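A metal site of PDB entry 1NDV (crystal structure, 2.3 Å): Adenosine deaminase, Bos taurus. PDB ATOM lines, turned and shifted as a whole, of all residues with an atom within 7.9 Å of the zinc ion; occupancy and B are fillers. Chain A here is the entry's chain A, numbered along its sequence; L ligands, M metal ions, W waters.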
ATOM      1  N   HIS A  14      12.179  26.106  28.910  1.00  0.00           N
ATOM      2  CA  HIS A  14      12.891  25.221  27.988  1.00  0.00           C
ATOM      3  C   HIS A  14      12.419  25.354  26.431  1.00  0.00           C
ATOM      4  O   HIS A  14      11.472  24.731  25.988  1.00  0.00           O
ATOM      5  CB  HIS A  14      12.685  23.789  28.563  1.00  0.00           C
ATOM      6  CG  HIS A  14      13.724  22.935  27.886  1.00  0.00           C
ATOM      7  ND1 HIS A  14      14.673  22.268  28.544  1.00  0.00           N
ATOM      8  CD2 HIS A  14      13.923  22.483  26.574  1.00  0.00           C
ATOM      9  CE1 HIS A  14      15.367  21.473  27.729  1.00  0.00           C
ATOM     10  NE2 HIS A  14      14.947  21.539  26.447  1.00  0.00           N
ATOM     11  N   VAL A  15      13.144  26.143  25.715  1.00  0.00           N
ATOM     12  CA  VAL A  15      12.938  26.240  24.324  1.00  0.00           C
ATOM     13  C   VAL A  15      14.221  26.777  23.712  1.00  0.00           C
ATOM     14  O   VAL A  15      14.872  27.690  24.239  1.00  0.00           O
ATOM     15  CB  VAL A  15      11.747  27.253  24.112  1.00  0.00           C
ATOM     16  CG1 VAL A  15      11.815  28.441  25.153  1.00  0.00           C
ATOM     17  CG2 VAL A  15      11.547  27.489  22.583  1.00  0.00           C
ATOM     18  N   HIS A  16      14.539  26.111  22.570  1.00  0.00           N
ATOM     19  CA  HIS A  16      15.814  26.402  21.879  1.00  0.00           C
ATOM     20  C   HIS A  16      15.648  27.462  20.696  1.00  0.00           C
ATOM     21  O   HIS A  16      14.974  27.115  19.711  1.00  0.00           O
ATOM     22  CB  HIS A  16      16.476  25.053  21.238  1.00  0.00           C
ATOM     23  CG  HIS A  16      16.816  23.870  22.210  1.00  0.00           C
ATOM     24  ND1 HIS A  16      18.096  23.622  22.521  1.00  0.00           N
ATOM     25  CD2 HIS A  16      16.052  22.901  22.876  1.00  0.00           C
ATOM     26  CE1 HIS A  16      18.196  22.519  23.336  1.00  0.00           C
ATOM     27  NE2 HIS A  16      16.927  22.030  23.582  1.00  0.00           N
ATOM     28  N   ARG A 100      17.103  29.475  24.988  1.00  0.00           N
ATOM     29  CA  ARG A 100      18.469  28.890  24.986  1.00  0.00           C
ATOM     30  C   ARG A 100      19.144  28.513  23.633  1.00  0.00           C
ATOM     31  O   ARG A 100      18.489  28.281  22.633  1.00  0.00           O
ATOM     32  CB  ARG A 100      18.611  27.565  25.888  1.00  0.00           C
ATOM     33  CG  ARG A 100      17.952  26.300  25.328  1.00  0.00           C
ATOM     34  CD  ARG A 100      17.716  25.173  26.336  1.00  0.00           C
ATOM     35  NE  ARG A 100      17.214  25.703  27.680  1.00  0.00           N
ATOM     36  CZ  ARG A 100      17.068  24.745  28.592  1.00  0.00           C
ATOM     37  NH1 ARG A 100      17.712  23.628  28.395  1.00  0.00           N
ATOM     38  NH2 ARG A 100      16.309  24.914  29.672  1.00  0.00           N
ATOM     39  N   CYS A 152      24.493  27.277  25.695  1.00  0.00           N
ATOM     40  CA  CYS A 152      24.303  25.822  25.819  1.00  0.00           C
ATOM     41  C   CYS A 152      25.661  25.057  25.527  1.00  0.00           C
ATOM     42  O   CYS A 152      25.961  24.986  24.341  1.00  0.00           O
ATOM     43  CB  CYS A 152      23.344  25.365  24.727  1.00  0.00           C
ATOM     44  SG  CYS A 152      21.592  25.469  24.994  1.00  0.00           S
ATOM     45  N   ASP A 180      23.632  25.781  30.047  1.00  0.00           N
ATOM     46  CA  ASP A 180      23.036  24.550  29.803  1.00  0.00           C
ATOM     47  C   ASP A 180      24.050  23.487  29.322  1.00  0.00           C
ATOM     48  O   ASP A 180      25.174  23.783  28.862  1.00  0.00           O
ATOM     49  CB  ASP A 180      21.706  24.606  29.041  1.00  0.00           C
ATOM     50  CG  ASP A 180      20.907  23.268  28.583  1.00  0.00           C
ATOM     51  OD1 ASP A 180      20.805  23.065  27.371  1.00  0.00           O
ATOM     52  OD2 ASP A 180      20.456  22.446  29.394  1.00  0.00           O
ATOM     53  N   LEU A 181      23.549  22.277  29.356  1.00  0.00           N
ATOM     54  CA  LEU A 181      24.202  21.191  28.684  1.00  0.00           C
ATOM     55  C   LEU A 181      23.266  20.389  27.748  1.00  0.00           C
ATOM     56  O   LEU A 181      22.314  19.721  28.149  1.00  0.00           O
ATOM     57  CB  LEU A 181      24.979  20.245  29.722  1.00  0.00           C
ATOM     58  CG  LEU A 181      25.700  19.014  29.016  1.00  0.00           C
ATOM     59  CD1 LEU A 181      26.752  19.391  27.865  1.00  0.00           C
ATOM     60  CD2 LEU A 181      26.735  18.418  30.014  1.00  0.00           C
ATOM     61  N   ALA A 182      23.686  20.499  26.531  1.00  0.00           N
ATOM     62  CA  ALA A 182      22.876  19.661  25.660  1.00  0.00           C
ATOM     63  C   ALA A 182      23.450  18.890  24.513  1.00  0.00           C
ATOM     64  O   ALA A 182      24.596  18.894  24.198  1.00  0.00           O
ATOM     65  CB  ALA A 182      21.846  20.490  24.904  1.00  0.00           C
ATOM     66  N   GLY A 183      22.565  18.157  23.918  1.00  0.00           N
ATOM     67  CA  GLY A 183      23.004  17.505  22.724  1.00  0.00           C
ATOM     68  C   GLY A 183      22.676  16.125  23.008  1.00  0.00           C
ATOM     69  O   GLY A 183      21.678  15.792  23.534  1.00  0.00           O
ATOM     70  N   HIS A 213      20.362  19.022  30.350  1.00  0.00           N
ATOM     71  CA  HIS A 213      19.414  18.156  29.756  1.00  0.00           C
ATOM     72  C   HIS A 213      19.771  16.692  30.171  1.00  0.00           C
ATOM     73  O   HIS A 213      20.893  16.314  30.022  1.00  0.00           O
ATOM     74  CB  HIS A 213      19.565  18.228  28.336  1.00  0.00           C
ATOM     75  CG  HIS A 213      18.864  19.312  27.594  1.00  0.00           C
ATOM     76  ND1 HIS A 213      19.465  20.547  27.441  1.00  0.00           N
ATOM     77  CD2 HIS A 213      17.818  19.142  26.633  1.00  0.00           C
ATOM     78  CE1 HIS A 213      18.889  21.057  26.410  1.00  0.00           C
ATOM     79  NE2 HIS A 213      17.908  20.273  25.868  1.00  0.00           N
ATOM     80  N   GLU A 216      15.965  12.247  29.359  1.00  0.00           N
ATOM     81  CA  GLU A 216      14.984  12.362  28.237  1.00  0.00           C
ATOM     82  C   GLU A 216      14.995  11.062  27.369  1.00  0.00           C
ATOM     83  O   GLU A 216      14.045  10.316  27.390  1.00  0.00           O
ATOM     84  CB  GLU A 216      15.324  13.642  27.397  1.00  0.00           C
ATOM     85  CG  GLU A 216      14.705  13.638  25.972  1.00  0.00           C
ATOM     86  CD  GLU A 216      15.324  14.631  25.008  1.00  0.00           C
ATOM     87  OE1 GLU A 216      16.488  15.038  25.159  1.00  0.00           O
ATOM     88  OE2 GLU A 216      14.571  14.950  24.073  1.00  0.00           O
ATOM     89  N   GLY A 236      16.510  19.827  32.382  1.00  0.00           N
ATOM     90  CA  GLY A 236      15.852  19.426  31.122  1.00  0.00           C
ATOM     91  C   GLY A 236      15.273  18.063  30.797  1.00  0.00           C
ATOM     92  O   GLY A 236      15.990  17.125  30.473  1.00  0.00           O
ATOM     93  N   HIS A 237      13.965  18.054  30.881  1.00  0.00           N
ATOM     94  CA  HIS A 237      13.080  16.917  30.959  1.00  0.00           C
ATOM     95  C   HIS A 237      12.999  15.944  32.267  1.00  0.00           C
ATOM     96  O   HIS A 237      12.017  15.797  33.018  1.00  0.00           O
ATOM     97  CB  HIS A 237      13.217  16.069  29.690  1.00  0.00           C
ATOM     98  CG  HIS A 237      13.442  16.740  28.371  1.00  0.00           C
ATOM     99  ND1 HIS A 237      12.422  17.033  27.513  1.00  0.00           N
ATOM    100  CD2 HIS A 237      14.630  16.968  27.706  1.00  0.00           C
ATOM    101  CE1 HIS A 237      12.893  17.394  26.301  1.00  0.00           C
ATOM    102  NE2 HIS A 237      14.251  17.323  26.498  1.00  0.00           N
ATOM    103  N   GLU A 259      11.862  20.695  33.740  1.00  0.00           N
ATOM    104  CA  GLU A 259      11.484  21.377  32.473  1.00  0.00           C
ATOM    105  C   GLU A 259      10.868  20.310  31.522  1.00  0.00           C
ATOM    106  O   GLU A 259      11.509  19.678  30.682  1.00  0.00           O
ATOM    107  CB  GLU A 259      12.774  21.883  31.762  1.00  0.00           C
ATOM    108  CG  GLU A 259      13.413  22.896  32.714  1.00  0.00           C
ATOM    109  CD  GLU A 259      14.797  23.364  32.307  1.00  0.00           C
ATOM    110  OE1 GLU A 259      15.153  22.958  31.248  1.00  0.00           O
ATOM    111  OE2 GLU A 259      15.456  24.162  32.947  1.00  0.00           O
ATOM    112  N   CYS A 261       8.999  18.935  28.301  1.00  0.00           N
ATOM    113  CA  CYS A 261       8.396  19.034  27.026  1.00  0.00           C
ATOM    114  C   CYS A 261       7.374  17.999  26.443  1.00  0.00           C
ATOM    115  O   CYS A 261       7.729  17.238  25.557  1.00  0.00           O
ATOM    116  CB  CYS A 261       9.520  19.209  26.106  1.00  0.00           C
ATOM    117  SG  CYS A 261      10.665  20.209  26.980  1.00  0.00           S
ATOM    118  N   SER A 264       7.133  17.392  22.592  1.00  0.00           N
ATOM    119  CA  SER A 264       8.441  16.708  22.437  1.00  0.00           C
ATOM    120  C   SER A 264       8.713  15.269  22.869  1.00  0.00           C
ATOM    121  O   SER A 264       9.179  14.457  22.116  1.00  0.00           O
ATOM    122  CB  SER A 264       9.524  17.471  23.009  1.00  0.00           C
ATOM    123  OG  SER A 264      10.509  17.361  21.996  1.00  0.00           O
ATOM    124  N   THR A 293       7.777  23.870  25.110  1.00  0.00           N
ATOM    125  CA  THR A 293       7.765  23.658  23.632  1.00  0.00           C
ATOM    126  C   THR A 293       8.953  22.979  23.050  1.00  0.00           C
ATOM    127  O   THR A 293       8.802  22.146  22.167  1.00  0.00           O
ATOM    128  CB  THR A 293       7.635  25.107  22.937  1.00  0.00           C
ATOM    129  OG1 THR A 293       6.382  25.419  22.416  1.00  0.00           O
ATOM    130  CG2 THR A 293       8.737  25.964  22.430  1.00  0.00           C
ATOM    131  N   ASP A 294      10.161  23.391  23.547  1.00  0.00           N
ATOM    132  CA  ASP A 294      11.382  22.917  22.974  1.00  0.00           C
ATOM    133  C   ASP A 294      11.986  23.206  21.658  1.00  0.00           C
ATOM    134  O   ASP A 294      12.943  23.941  21.478  1.00  0.00           O
ATOM    135  CB  ASP A 294      11.309  21.411  23.088  1.00  0.00           C
ATOM    136  CG  ASP A 294      12.669  20.706  23.320  1.00  0.00           C
ATOM    137  OD1 ASP A 294      12.629  19.487  23.582  1.00  0.00           O
ATOM    138  OD2 ASP A 294      13.703  21.395  23.257  1.00  0.00           O
ATOM    139  N   ASP A 295      11.464  22.445  20.689  1.00  0.00           N
ATOM    140  CA  ASP A 295      11.936  22.778  19.303  1.00  0.00           C
ATOM    141  C   ASP A 295      10.743  23.026  18.348  1.00  0.00           C
ATOM    142  O   ASP A 295      10.359  22.195  17.514  1.00  0.00           O
ATOM    143  CB  ASP A 295      12.731  21.721  18.594  1.00  0.00           C
ATOM    144  CG  ASP A 295      14.168  21.778  19.046  1.00  0.00           C
ATOM    145  OD1 ASP A 295      14.976  22.639  18.632  1.00  0.00           O
ATOM    146  OD2 ASP A 295      14.449  20.909  19.846  1.00  0.00           O
ATOM    147  N   PHE A 299       8.826  20.617  15.711  1.00  0.00           N
ATOM    148  CA  PHE A 299       7.654  19.837  16.201  1.00  0.00           C
ATOM    149  C   PHE A 299       6.218  20.190  15.765  1.00  0.00           C
ATOM    150  O   PHE A 299       5.237  19.664  16.299  1.00  0.00           O
ATOM    151  CB  PHE A 299       7.719  19.671  17.726  1.00  0.00           C
ATOM    152  CG  PHE A 299       9.085  19.198  18.105  1.00  0.00           C
ATOM    153  CD1 PHE A 299       9.894  18.360  17.252  1.00  0.00           C
ATOM    154  CD2 PHE A 299       9.566  19.626  19.376  1.00  0.00           C
ATOM    155  CE1 PHE A 299      11.156  17.917  17.704  1.00  0.00           C
ATOM    156  CE2 PHE A 299      10.829  19.141  19.855  1.00  0.00           C
ATOM    157  CZ  PHE A 299      11.556  18.239  19.041  1.00  0.00           C
HETATM  158  N1  LIG L   1      16.479  11.795  19.855  1.00  0.00           N
HETATM  159  C1  LIG L   1      15.479  12.111  18.959  1.00  0.00           C
HETATM  160  C2  LIG L   1      15.274  13.516  19.092  1.00  0.00           C
HETATM  161  N2  LIG L   1      16.175  13.961  20.046  1.00  0.00           N
HETATM  162  C3  LIG L   1      16.840  12.921  20.482  1.00  0.00           C
HETATM  163  C4  LIG L   1      14.693  11.364  18.077  1.00  0.00           C
HETATM  164  C5  LIG L   1      13.713  12.061  17.327  1.00  0.00           C
HETATM  165  C6  LIG L   1      13.501  13.461  17.463  1.00  0.00           C
HETATM  166  C7  LIG L   1      14.293  14.196  18.340  1.00  0.00           C
HETATM  167  N3  LIG L   1      17.741  12.997  21.655  1.00  0.00           N
HETATM  168  C8  LIG L   1      18.008  14.251  22.350  1.00  0.00           C
HETATM  169  C9  LIG L   1      18.840  15.077  21.456  1.00  0.00           C
HETATM  170  S1  LIG L   1      18.635  16.750  21.137  1.00  0.00           S
HETATM  171  C10 LIG L   1      20.117  16.805  20.095  1.00  0.00           C
HETATM  172  C11 LIG L   1      20.683  15.467  19.970  1.00  0.00           C
HETATM  173  C12 LIG L   1      19.943  14.486  20.741  1.00  0.00           C
HETATM  174  C13 LIG L   1      20.715  17.806  19.413  1.00  0.00           C
HETATM  175  N4  LIG L   1      19.999  19.047  19.861  1.00  0.00           N
HETATM  176  C14 LIG L   1      20.443  20.281  19.498  1.00  0.00           C
HETATM  177  S2  LIG L   1      21.711  19.977  18.336  1.00  0.00           S
HETATM  178  C15 LIG L   1      21.585  18.298  18.538  1.00  0.00           C
HETATM  179  N5  LIG L   1      19.855  21.499  19.655  1.00  0.00           N
HETATM  180  C16 LIG L   1      18.499  21.676  19.674  1.00  0.00           C
HETATM  181  N6  LIG L   1      17.730  20.793  20.248  1.00  0.00           N
HETATM  182  N7  LIG L   1      17.883  22.705  19.091  1.00  0.00           N
HETATM  183 ZN    ZN M   1      16.031  20.932  24.854  1.00  0.00          ZN
HETATM  184  O   HOH W   1      14.757  19.408  25.183  1.00  0.00           O
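The zinc ion is bound by a ring nitrogen (NE2) of His 16 (1.9 Å), water W1 (2.0 Å), a ring nitrogen (NE2) of His 14 (2.0 Å) and a ring nitrogen (NE2) of His 213 (2.2 Å).
OD1 of Asp 295 is in salt-bridge range of N7 of the ligand, 2.9 Å away.
Water W1 bridges a ring nitrogen (NE2) of His 237 (2.5 Å) and the side-chain carboxylate (OD1) of Asp 294 (2.7 Å).
The backbone NH (N) of His 16 is in hydrogen-bond range of the backbone carbonyl oxygen (O) of Asp 294, at 2.9 Å. N of Asp 294 is in hydrogen-bond range of O of His 14 (3.1 Å). A ring nitrogen (ND1) of His 14 sits at hydrogen-bond distance from the guanidinium group (NH2) of Arg 100, 3.3 Å away. A ring nitrogen (ND1) of His 14 is in hydrogen-bond range of the side-chain carboxylate of Glu 259, 2.8 Å away. ND1 of His 213 lies within hydrogen-bond range of OD1 of Asp 180, 2.9 Å away. The backbone NH of His 213 is in hydrogen-bond range of the backbone carbonyl oxygen of Leu 181 (3.0 Å). OG of Ser 264 is in hydrogen-bond range of OD1 of Asp 294 (3.4 Å).
Residues that only touch the zinc ion: Asp 294 (2.9 Å). Four residues have an atom within 4 Å of the zinc ion: His 14, His 16, His 213 and Asp 294.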
